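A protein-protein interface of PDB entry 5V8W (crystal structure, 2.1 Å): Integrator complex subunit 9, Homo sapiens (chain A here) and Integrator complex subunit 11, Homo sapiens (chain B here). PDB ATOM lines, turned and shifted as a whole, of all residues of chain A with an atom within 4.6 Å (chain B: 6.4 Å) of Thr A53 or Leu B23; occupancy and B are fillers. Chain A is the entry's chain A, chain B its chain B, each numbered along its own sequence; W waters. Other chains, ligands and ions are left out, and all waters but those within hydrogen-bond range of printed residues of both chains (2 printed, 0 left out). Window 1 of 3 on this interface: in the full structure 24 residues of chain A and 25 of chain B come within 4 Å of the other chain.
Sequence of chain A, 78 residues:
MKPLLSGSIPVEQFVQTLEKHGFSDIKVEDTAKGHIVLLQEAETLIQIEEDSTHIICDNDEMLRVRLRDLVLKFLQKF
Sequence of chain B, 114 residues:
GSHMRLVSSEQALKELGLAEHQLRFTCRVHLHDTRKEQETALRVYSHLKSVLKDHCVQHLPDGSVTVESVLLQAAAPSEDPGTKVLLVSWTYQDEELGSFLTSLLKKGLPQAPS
Of the 9 printed residues of chain B, 6 touch a printed residue of chain A. Printed residues of chain B that touch a printed residue of chain A: His B21, Gln B22, Leu B23, Arg B24, Phe B25 and Tyr B92. Hydrophobic or aromatic side chains of chain B that line the printed part of chain A: His B21, Leu B23, Phe B25 and Tyr B92. Printed residues of chain A that touch a printed residue of chain B: Leu A5, Asp A51, Ser A52, Thr A53, His A54, Ile A55, Val A71 and Leu A72. Among the printed residues, 18 pairs touch across the chains. Among the printed residues, no Asp or Glu carboxylate lies within 4 Å of a Lys or Arg side-chain nitrogen of the other chain.
N of Tyr B92 lies within hydrogen-bond range of O of Leu B23 (2.9 Å). N of Gln A47 lies within hydrogen-bond range of O of His A54 (2.9 Å). The backbone NH (N) of Phe B25 sits at hydrogen-bond distance from the backbone carbonyl oxygen (O) of Trp B90, at 2.8 Å.
Of the printed residues of chain B, Leu A5 touches His B21, Leu B23 and Tyr B92. Ile A9 touches none of the printed residues of chain B. Thr A53 touches four residues of chain B. Of the printed residues of chain A, His B21 touches Leu A5 (2.8 Å), Asp A51 (3.5 Å), Ser A52 (3.7 Å) and Thr A53 (2.6 Å). Of the printed residues of chain A, Gln B22 touches Asp A51 (2.8 Å), Ser A52 (3.5 Å) and Thr A53 (2.9 Å). Leu B23 touches four residues of chain A. Of the printed residues of chain A, Phe B25 touches His A54 (3.8 Å) and Ile A55 (3.3 Å). The nearest residue of chain A that does not touch Leu B23 is Ile A55 (4.4 Å).
The backbone carbonyl oxygen of Thr A53 is in hydrogen-bond range of the backbone NH of Arg B24, at 2.9 Å. N of Ile A55 lies within hydrogen-bond range of O of Arg B24, at 2.8 Å. The backbone carbonyl oxygen (O) of Asp A51 is in hydrogen-bond range of the backbone NH (N) of Gln B22 (2.8 Å). The backbone carbonyl oxygen of Gln B22 sits at hydrogen-bond distance from the backbone NH of Thr A53 (2.9 Å). O of Leu A5 sits at hydrogen-bond distance from N of His B21, 2.8 Å away. The side-chain hydroxyl of Thr A53 sits at hydrogen-bond distance from a ring nitrogen (NE2) of His B21.
Water W2 lies within hydrogen-bond range of OE1 of Gln B22 (2.7 Å), OG of Ser A52 (2.7 Å) and O of Thr A53 (3.2 Å). Water W1 lies within hydrogen-bond range of the backbone carbonyl oxygen of His B21 (2.7 Å) and the backbone NH of Leu A5 (3.0 Å).
Among the printed residues, pairs that only touch across the chains: Ile A55 with Phe B25, His A54 with Arg B24, Leu A72 with Tyr B92, Ser A52 with Gln B22, Asp A51 with His B21, Thr A53 with Leu B23, Ser A52 with His B21, Leu A5 with Tyr B92, His A54 with Phe B25, Leu A5 with Leu B23, Leu A72 with Leu B23 and Val A71 with Leu B23.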
ATOM      1  N   LEU A   5      19.016 -12.146  -9.852  1.00  0.00           N
ATOM      2  CA  LEU A   5      20.340 -11.589  -9.555  1.00  0.00           C
ATOM      3  C   LEU A   5      21.062 -11.286 -10.856  1.00  0.00           C
ATOM      4  O   LEU A   5      20.842 -11.963 -11.855  1.00  0.00           O
ATOM      5  CB  LEU A   5      21.184 -12.578  -8.723  1.00  0.00           C
ATOM      6  CG  LEU A   5      20.589 -13.044  -7.400  1.00  0.00           C
ATOM      7  CD1 LEU A   5      21.406 -14.209  -6.807  1.00  0.00           C
ATOM      8  CD2 LEU A   5      20.536 -11.847  -6.420  1.00  0.00           C
ATOM      9  N   ILE A   9      31.313 -11.152  -9.759  1.00  0.00           N
ATOM     10  CA  ILE A   9      32.047 -11.217  -8.502  1.00  0.00           C
ATOM     11  C   ILE A   9      33.533 -11.100  -8.800  1.00  0.00           C
ATOM     12  O   ILE A   9      34.122 -12.040  -9.316  1.00  0.00           O
ATOM     13  CB  ILE A   9      31.798 -12.537  -7.756  1.00  0.00           C
ATOM     14  CG1 ILE A   9      30.316 -12.677  -7.398  1.00  0.00           C
ATOM     15  CG2 ILE A   9      32.675 -12.616  -6.512  1.00  0.00           C
ATOM     16  CD1 ILE A   9      30.062 -13.894  -6.663  1.00  0.00           C
ATOM     17  N   ILE A  46      34.174 -22.358  -4.020  1.00  0.00           N
ATOM     18  CA  ILE A  46      33.316 -21.347  -4.603  1.00  0.00           C
ATOM     19  C   ILE A  46      33.785 -21.133  -6.056  1.00  0.00           C
ATOM     20  O   ILE A  46      34.816 -20.528  -6.294  1.00  0.00           O
ATOM     21  CB  ILE A  46      33.391 -20.036  -3.848  1.00  0.00           C
ATOM     22  CG1 ILE A  46      33.154 -20.275  -2.366  1.00  0.00           C
ATOM     23  CG2 ILE A  46      32.403 -19.028  -4.453  1.00  0.00           C
ATOM     24  CD1 ILE A  46      33.450 -19.106  -1.507  1.00  0.00           C
ATOM     25  N   GLN A  47      33.048 -21.677  -7.004  1.00  0.00           N
ATOM     26  CA  GLN A  47      33.367 -21.540  -8.426  1.00  0.00           C
ATOM     27  C   GLN A  47      32.836 -20.232  -8.952  1.00  0.00           C
ATOM     28  O   GLN A  47      31.620 -20.006  -8.945  1.00  0.00           O
ATOM     29  CB  GLN A  47      32.771 -22.675  -9.233  1.00  0.00           C
ATOM     30  CG  GLN A  47      33.125 -24.062  -8.664  1.00  0.00           C
ATOM     31  CD  GLN A  47      32.387 -25.210  -9.393  1.00  0.00           C
ATOM     32  OE1 GLN A  47      31.245 -25.059  -9.838  1.00  0.00           O
ATOM     33  NE2 GLN A  47      33.031 -26.359  -9.480  1.00  0.00           N
ATOM     34  N   ASP A  51      28.485 -14.758 -14.912  1.00  0.00           N
ATOM     35  CA  ASP A  51      27.077 -15.017 -14.613  1.00  0.00           C
ATOM     36  C   ASP A  51      26.809 -16.314 -13.847  1.00  0.00           C
ATOM     37  O   ASP A  51      25.673 -16.819 -13.855  1.00  0.00           O
ATOM     38  CB  ASP A  51      26.270 -15.039 -15.916  1.00  0.00           C
ATOM     39  CG  ASP A  51      26.527 -13.818 -16.757  1.00  0.00           C
ATOM     40  OD1 ASP A  51      26.760 -12.760 -16.138  1.00  0.00           O
ATOM     41  OD2 ASP A  51      26.501 -13.910 -18.016  1.00  0.00           O
ATOM     42  N   SER A  52      27.827 -16.862 -13.192  1.00  0.00           N
ATOM     43  CA  SER A  52      27.635 -18.119 -12.468  1.00  0.00           C
ATOM     44  C   SER A  52      28.516 -18.255 -11.229  1.00  0.00           C
ATOM     45  O   SER A  52      29.728 -18.289 -11.314  1.00  0.00           O
ATOM     46  CB  SER A  52      27.883 -19.310 -13.407  1.00  0.00           C
ATOM     47  OG  SER A  52      27.939 -20.528 -12.656  1.00  0.00           O
ATOM     48  N   THR A  53      27.894 -18.354 -10.068  1.00  0.00           N
ATOM     49  CA  THR A  53      28.639 -18.607  -8.856  1.00  0.00           C
ATOM     50  C   THR A  53      28.104 -19.893  -8.244  1.00  0.00           C
ATOM     51  O   THR A  53      26.893 -20.034  -8.052  1.00  0.00           O
ATOM     52  CB  THR A  53      28.505 -17.447  -7.827  1.00  0.00           C
ATOM     53  OG1 THR A  53      28.844 -16.196  -8.437  1.00  0.00           O
ATOM     54  CG2 THR A  53      29.396 -17.713  -6.571  1.00  0.00           C
ATOM     55  N   HIS A  54      28.983 -20.821  -7.904  1.00  0.00           N
ATOM     56  CA  HIS A  54      28.499 -22.101  -7.389  1.00  0.00           C
ATOM     57  C   HIS A  54      29.257 -22.422  -6.112  1.00  0.00           C
ATOM     58  O   HIS A  54      30.466 -22.617  -6.126  1.00  0.00           O
ATOM     59  CB  HIS A  54      28.659 -23.238  -8.419  1.00  0.00           C
ATOM     60  CG  HIS A  54      27.985 -24.534  -8.030  1.00  0.00           C
ATOM     61  ND1 HIS A  54      27.872 -25.599  -8.905  1.00  0.00           N
ATOM     62  CD2 HIS A  54      27.340 -24.914  -6.894  1.00  0.00           C
ATOM     63  CE1 HIS A  54      27.227 -26.593  -8.313  1.00  0.00           C
ATOM     64  NE2 HIS A  54      26.881 -26.200  -7.097  1.00  0.00           N
ATOM     65  N   ILE A  55      28.524 -22.437  -5.011  1.00  0.00           N
ATOM     66  CA  ILE A  55      29.088 -22.753  -3.712  1.00  0.00           C
ATOM     67  C   ILE A  55      28.840 -24.233  -3.415  1.00  0.00           C
ATOM     68  O   ILE A  55      27.674 -24.684  -3.351  1.00  0.00           O
ATOM     69  CB  ILE A  55      28.475 -21.868  -2.607  1.00  0.00           C
ATOM     70  CG1 ILE A  55      28.874 -20.384  -2.824  1.00  0.00           C
ATOM     71  CG2 ILE A  55      28.856 -22.391  -1.216  1.00  0.00           C
ATOM     72  CD1 ILE A  55      28.131 -19.370  -1.894  1.00  0.00           C
ATOM     73  N   VAL A  71      28.399 -13.217  -1.099  1.00  0.00           N
ATOM     74  CA  VAL A  71      28.229 -13.258  -2.552  1.00  0.00           C
ATOM     75  C   VAL A  71      27.113 -12.298  -2.992  1.00  0.00           C
ATOM     76  O   VAL A  71      27.303 -11.527  -3.926  1.00  0.00           O
ATOM     77  CB  VAL A  71      27.924 -14.670  -3.043  1.00  0.00           C
ATOM     78  CG1 VAL A  71      27.370 -14.638  -4.483  1.00  0.00           C
ATOM     79  CG2 VAL A  71      29.196 -15.516  -2.961  1.00  0.00           C
ATOM     80  N   LEU A  72      25.979 -12.316  -2.280  1.00  0.00           N
ATOM     81  CA  LEU A  72      24.831 -11.456  -2.603  1.00  0.00           C
ATOM     82  C   LEU A  72      25.158  -9.955  -2.540  1.00  0.00           C
ATOM     83  O   LEU A  72      24.584  -9.173  -3.303  1.00  0.00           O
ATOM     84  CB  LEU A  72      23.647 -11.765  -1.676  1.00  0.00           C
ATOM     85  CG  LEU A  72      22.966 -13.120  -1.951  1.00  0.00           C
ATOM     86  CD1 LEU A  72      21.946 -13.483  -0.844  1.00  0.00           C
ATOM     87  CD2 LEU A  72      22.300 -13.110  -3.341  1.00  0.00           C
ATOM     88  N   HIS B  21      22.414 -13.715 -13.292  1.00  0.00           N
ATOM     89  CA  HIS B  21      23.497 -14.388 -12.575  1.00  0.00           C
ATOM     90  C   HIS B  21      22.891 -15.577 -11.868  1.00  0.00           C
ATOM     91  O   HIS B  21      21.974 -15.390 -11.055  1.00  0.00           O
ATOM     92  CB  HIS B  21      24.167 -13.447 -11.558  1.00  0.00           C
ATOM     93  CG  HIS B  21      25.482 -13.948 -11.020  1.00  0.00           C
ATOM     94  ND1 HIS B  21      26.698 -13.470 -11.469  1.00  0.00           N
ATOM     95  CD2 HIS B  21      25.768 -14.865 -10.059  1.00  0.00           C
ATOM     96  CE1 HIS B  21      27.678 -14.087 -10.822  1.00  0.00           C
ATOM     97  NE2 HIS B  21      27.143 -14.938  -9.959  1.00  0.00           N
ATOM     98  N   GLN B  22      23.382 -16.786 -12.165  1.00  0.00           N
ATOM     99  CA  GLN B  22      22.910 -17.987 -11.467  1.00  0.00           C
ATOM    100  C   GLN B  22      23.739 -18.182 -10.209  1.00  0.00           C
ATOM    101  O   GLN B  22      24.953 -18.362 -10.287  1.00  0.00           O
ATOM    102  CB  GLN B  22      22.984 -19.241 -12.366  1.00  0.00           C
ATOM    103  CG  GLN B  22      22.482 -20.546 -11.658  1.00  0.00           C
ATOM    104  CD  GLN B  22      22.875 -21.898 -12.353  1.00  0.00           C
ATOM    105  OE1 GLN B  22      24.054 -22.258 -12.446  1.00  0.00           O
ATOM    106  NE2 GLN B  22      21.868 -22.654 -12.785  1.00  0.00           N
ATOM    107  N   LEU B  23      23.090 -18.115  -9.045  1.00  0.00           N
ATOM    108  CA  LEU B  23      23.752 -18.478  -7.797  1.00  0.00           C
ATOM    109  C   LEU B  23      23.293 -19.861  -7.357  1.00  0.00           C
ATOM    110  O   LEU B  23      22.122 -20.076  -7.039  1.00  0.00           O
ATOM    111  CB  LEU B  23      23.470 -17.460  -6.695  1.00  0.00           C
ATOM    112  CG  LEU B  23      23.952 -17.791  -5.271  1.00  0.00           C
ATOM    113  CD1 LEU B  23      25.461 -18.015  -5.158  1.00  0.00           C
ATOM    114  CD2 LEU B  23      23.517 -16.676  -4.300  1.00  0.00           C
ATOM    115  N   ARG B  24      24.241 -20.783  -7.310  1.00  0.00           N
ATOM    116  CA  ARG B  24      23.917 -22.191  -7.083  1.00  0.00           C
ATOM    117  C   ARG B  24      24.647 -22.710  -5.838  1.00  0.00           C
ATOM    118  O   ARG B  24      25.773 -22.275  -5.537  1.00  0.00           O
ATOM    119  CB  ARG B  24      24.274 -23.014  -8.333  1.00  0.00           C
ATOM    120  CG  ARG B  24      24.012 -24.523  -8.226  1.00  0.00           C
ATOM    121  CD  ARG B  24      24.184 -25.234  -9.586  1.00  0.00           C
ATOM    122  NE  ARG B  24      24.046 -26.685  -9.433  1.00  0.00           N
ATOM    123  CZ  ARG B  24      24.429 -27.583 -10.342  1.00  0.00           C
ATOM    124  NH1 ARG B  24      24.980 -27.199 -11.502  1.00  0.00           N
ATOM    125  NH2 ARG B  24      24.256 -28.869 -10.084  1.00  0.00           N
ATOM    126  N   PHE B  25      23.964 -23.609  -5.125  1.00  0.00           N
ATOM    127  CA  PHE B  25      24.464 -24.258  -3.932  1.00  0.00           C
ATOM    128  C   PHE B  25      24.435 -25.763  -4.181  1.00  0.00           C
ATOM    129  O   PHE B  25      23.468 -26.273  -4.754  1.00  0.00           O
ATOM    130  CB  PHE B  25      23.594 -23.914  -2.699  1.00  0.00           C
ATOM    131  CG  PHE B  25      23.610 -22.455  -2.349  1.00  0.00           C
ATOM    132  CD1 PHE B  25      24.659 -21.920  -1.634  1.00  0.00           C
ATOM    133  CD2 PHE B  25      22.612 -21.626  -2.765  1.00  0.00           C
ATOM    134  CE1 PHE B  25      24.697 -20.571  -1.345  1.00  0.00           C
ATOM    135  CE2 PHE B  25      22.646 -20.262  -2.460  1.00  0.00           C
ATOM    136  CZ  PHE B  25      23.687 -19.750  -1.759  1.00  0.00           C
ATOM    137  N   TRP B  90      20.626 -26.600  -5.373  1.00  0.00           N
ATOM    138  CA  TRP B  90      19.539 -25.674  -5.711  1.00  0.00           C
ATOM    139  C   TRP B  90      20.128 -24.335  -6.103  1.00  0.00           C
ATOM    140  O   TRP B  90      21.283 -24.045  -5.774  1.00  0.00           O
ATOM    141  CB  TRP B  90      18.562 -25.485  -4.538  1.00  0.00           C
ATOM    142  CG  TRP B  90      19.145 -24.780  -3.301  1.00  0.00           C
ATOM    143  CD1 TRP B  90      18.963 -23.485  -2.960  1.00  0.00           C
ATOM    144  CD2 TRP B  90      19.980 -25.353  -2.268  1.00  0.00           C
ATOM    145  NE1 TRP B  90      19.600 -23.212  -1.786  1.00  0.00           N
ATOM    146  CE2 TRP B  90      20.229 -24.338  -1.334  1.00  0.00           C
ATOM    147  CE3 TRP B  90      20.497 -26.629  -2.030  1.00  0.00           C
ATOM    148  CZ2 TRP B  90      21.005 -24.549  -0.169  1.00  0.00           C
ATOM    149  CZ3 TRP B  90      21.275 -26.846  -0.872  1.00  0.00           C
ATOM    150  CH2 TRP B  90      21.517 -25.812   0.040  1.00  0.00           C
ATOM    151  N   THR B  91      19.355 -23.545  -6.843  1.00  0.00           N
ATOM    152  CA  THR B  91      19.720 -22.163  -7.079  1.00  0.00           C
ATOM    153  C   THR B  91      19.024 -21.267  -6.045  1.00  0.00           C
ATOM    154  O   THR B  91      18.131 -21.697  -5.278  1.00  0.00           O
ATOM    155  CB  THR B  91      19.343 -21.688  -8.492  1.00  0.00           C
ATOM    156  OG1 THR B  91      17.928 -21.537  -8.564  1.00  0.00           O
ATOM    157  CG2 THR B  91      19.793 -22.664  -9.549  1.00  0.00           C
ATOM    158  N   TYR B  92      19.448 -20.013  -6.049  1.00  0.00           N
ATOM    159  CA  TYR B  92      18.980 -19.011  -5.117  1.00  0.00           C
ATOM    160  C   TYR B  92      17.446 -18.834  -5.155  1.00  0.00           C
ATOM    161  O   TYR B  92      16.850 -18.603  -4.107  1.00  0.00           O
ATOM    162  CB  TYR B  92      19.699 -17.677  -5.380  1.00  0.00           C
ATOM    163  CG  TYR B  92      19.410 -16.680  -4.292  1.00  0.00           C
ATOM    164  CD1 TYR B  92      19.758 -16.967  -2.974  1.00  0.00           C
ATOM    165  CD2 TYR B  92      18.755 -15.482  -4.560  1.00  0.00           C
ATOM    166  CE1 TYR B  92      19.480 -16.082  -1.953  1.00  0.00           C
ATOM    167  CE2 TYR B  92      18.475 -14.576  -3.537  1.00  0.00           C
ATOM    168  CZ  TYR B  92      18.841 -14.887  -2.233  1.00  0.00           C
ATOM    169  OH  TYR B  92      18.581 -14.032  -1.193  1.00  0.00           O
ATOM    170  N   GLN B  93      16.817 -18.985  -6.327  1.00  0.00           N
ATOM    171  CA  GLN B  93      15.347 -19.012  -6.442  1.00  0.00           C
ATOM    172  C   GLN B  93      14.675 -19.934  -5.420  1.00  0.00           C
ATOM    173  O   GLN B  93      13.576 -19.642  -4.912  1.00  0.00           O
ATOM    174  CB  GLN B  93      14.893 -19.472  -7.840  1.00  0.00           C
ATOM    175  CG  GLN B  93      15.207 -18.526  -8.963  1.00  0.00           C
ATOM    176  CD  GLN B  93      15.034 -17.075  -8.565  1.00  0.00           C
ATOM    177  OE1 GLN B  93      16.021 -16.345  -8.372  1.00  0.00           O
ATOM    178  NE2 GLN B  93      13.773 -16.642  -8.431  1.00  0.00           N
HETATM  179  O   HOH W   1      19.393 -15.032 -10.374  1.00  0.00           O
HETATM  180  O   HOH W   2      25.968 -21.275 -10.894  1.00  0.00           O
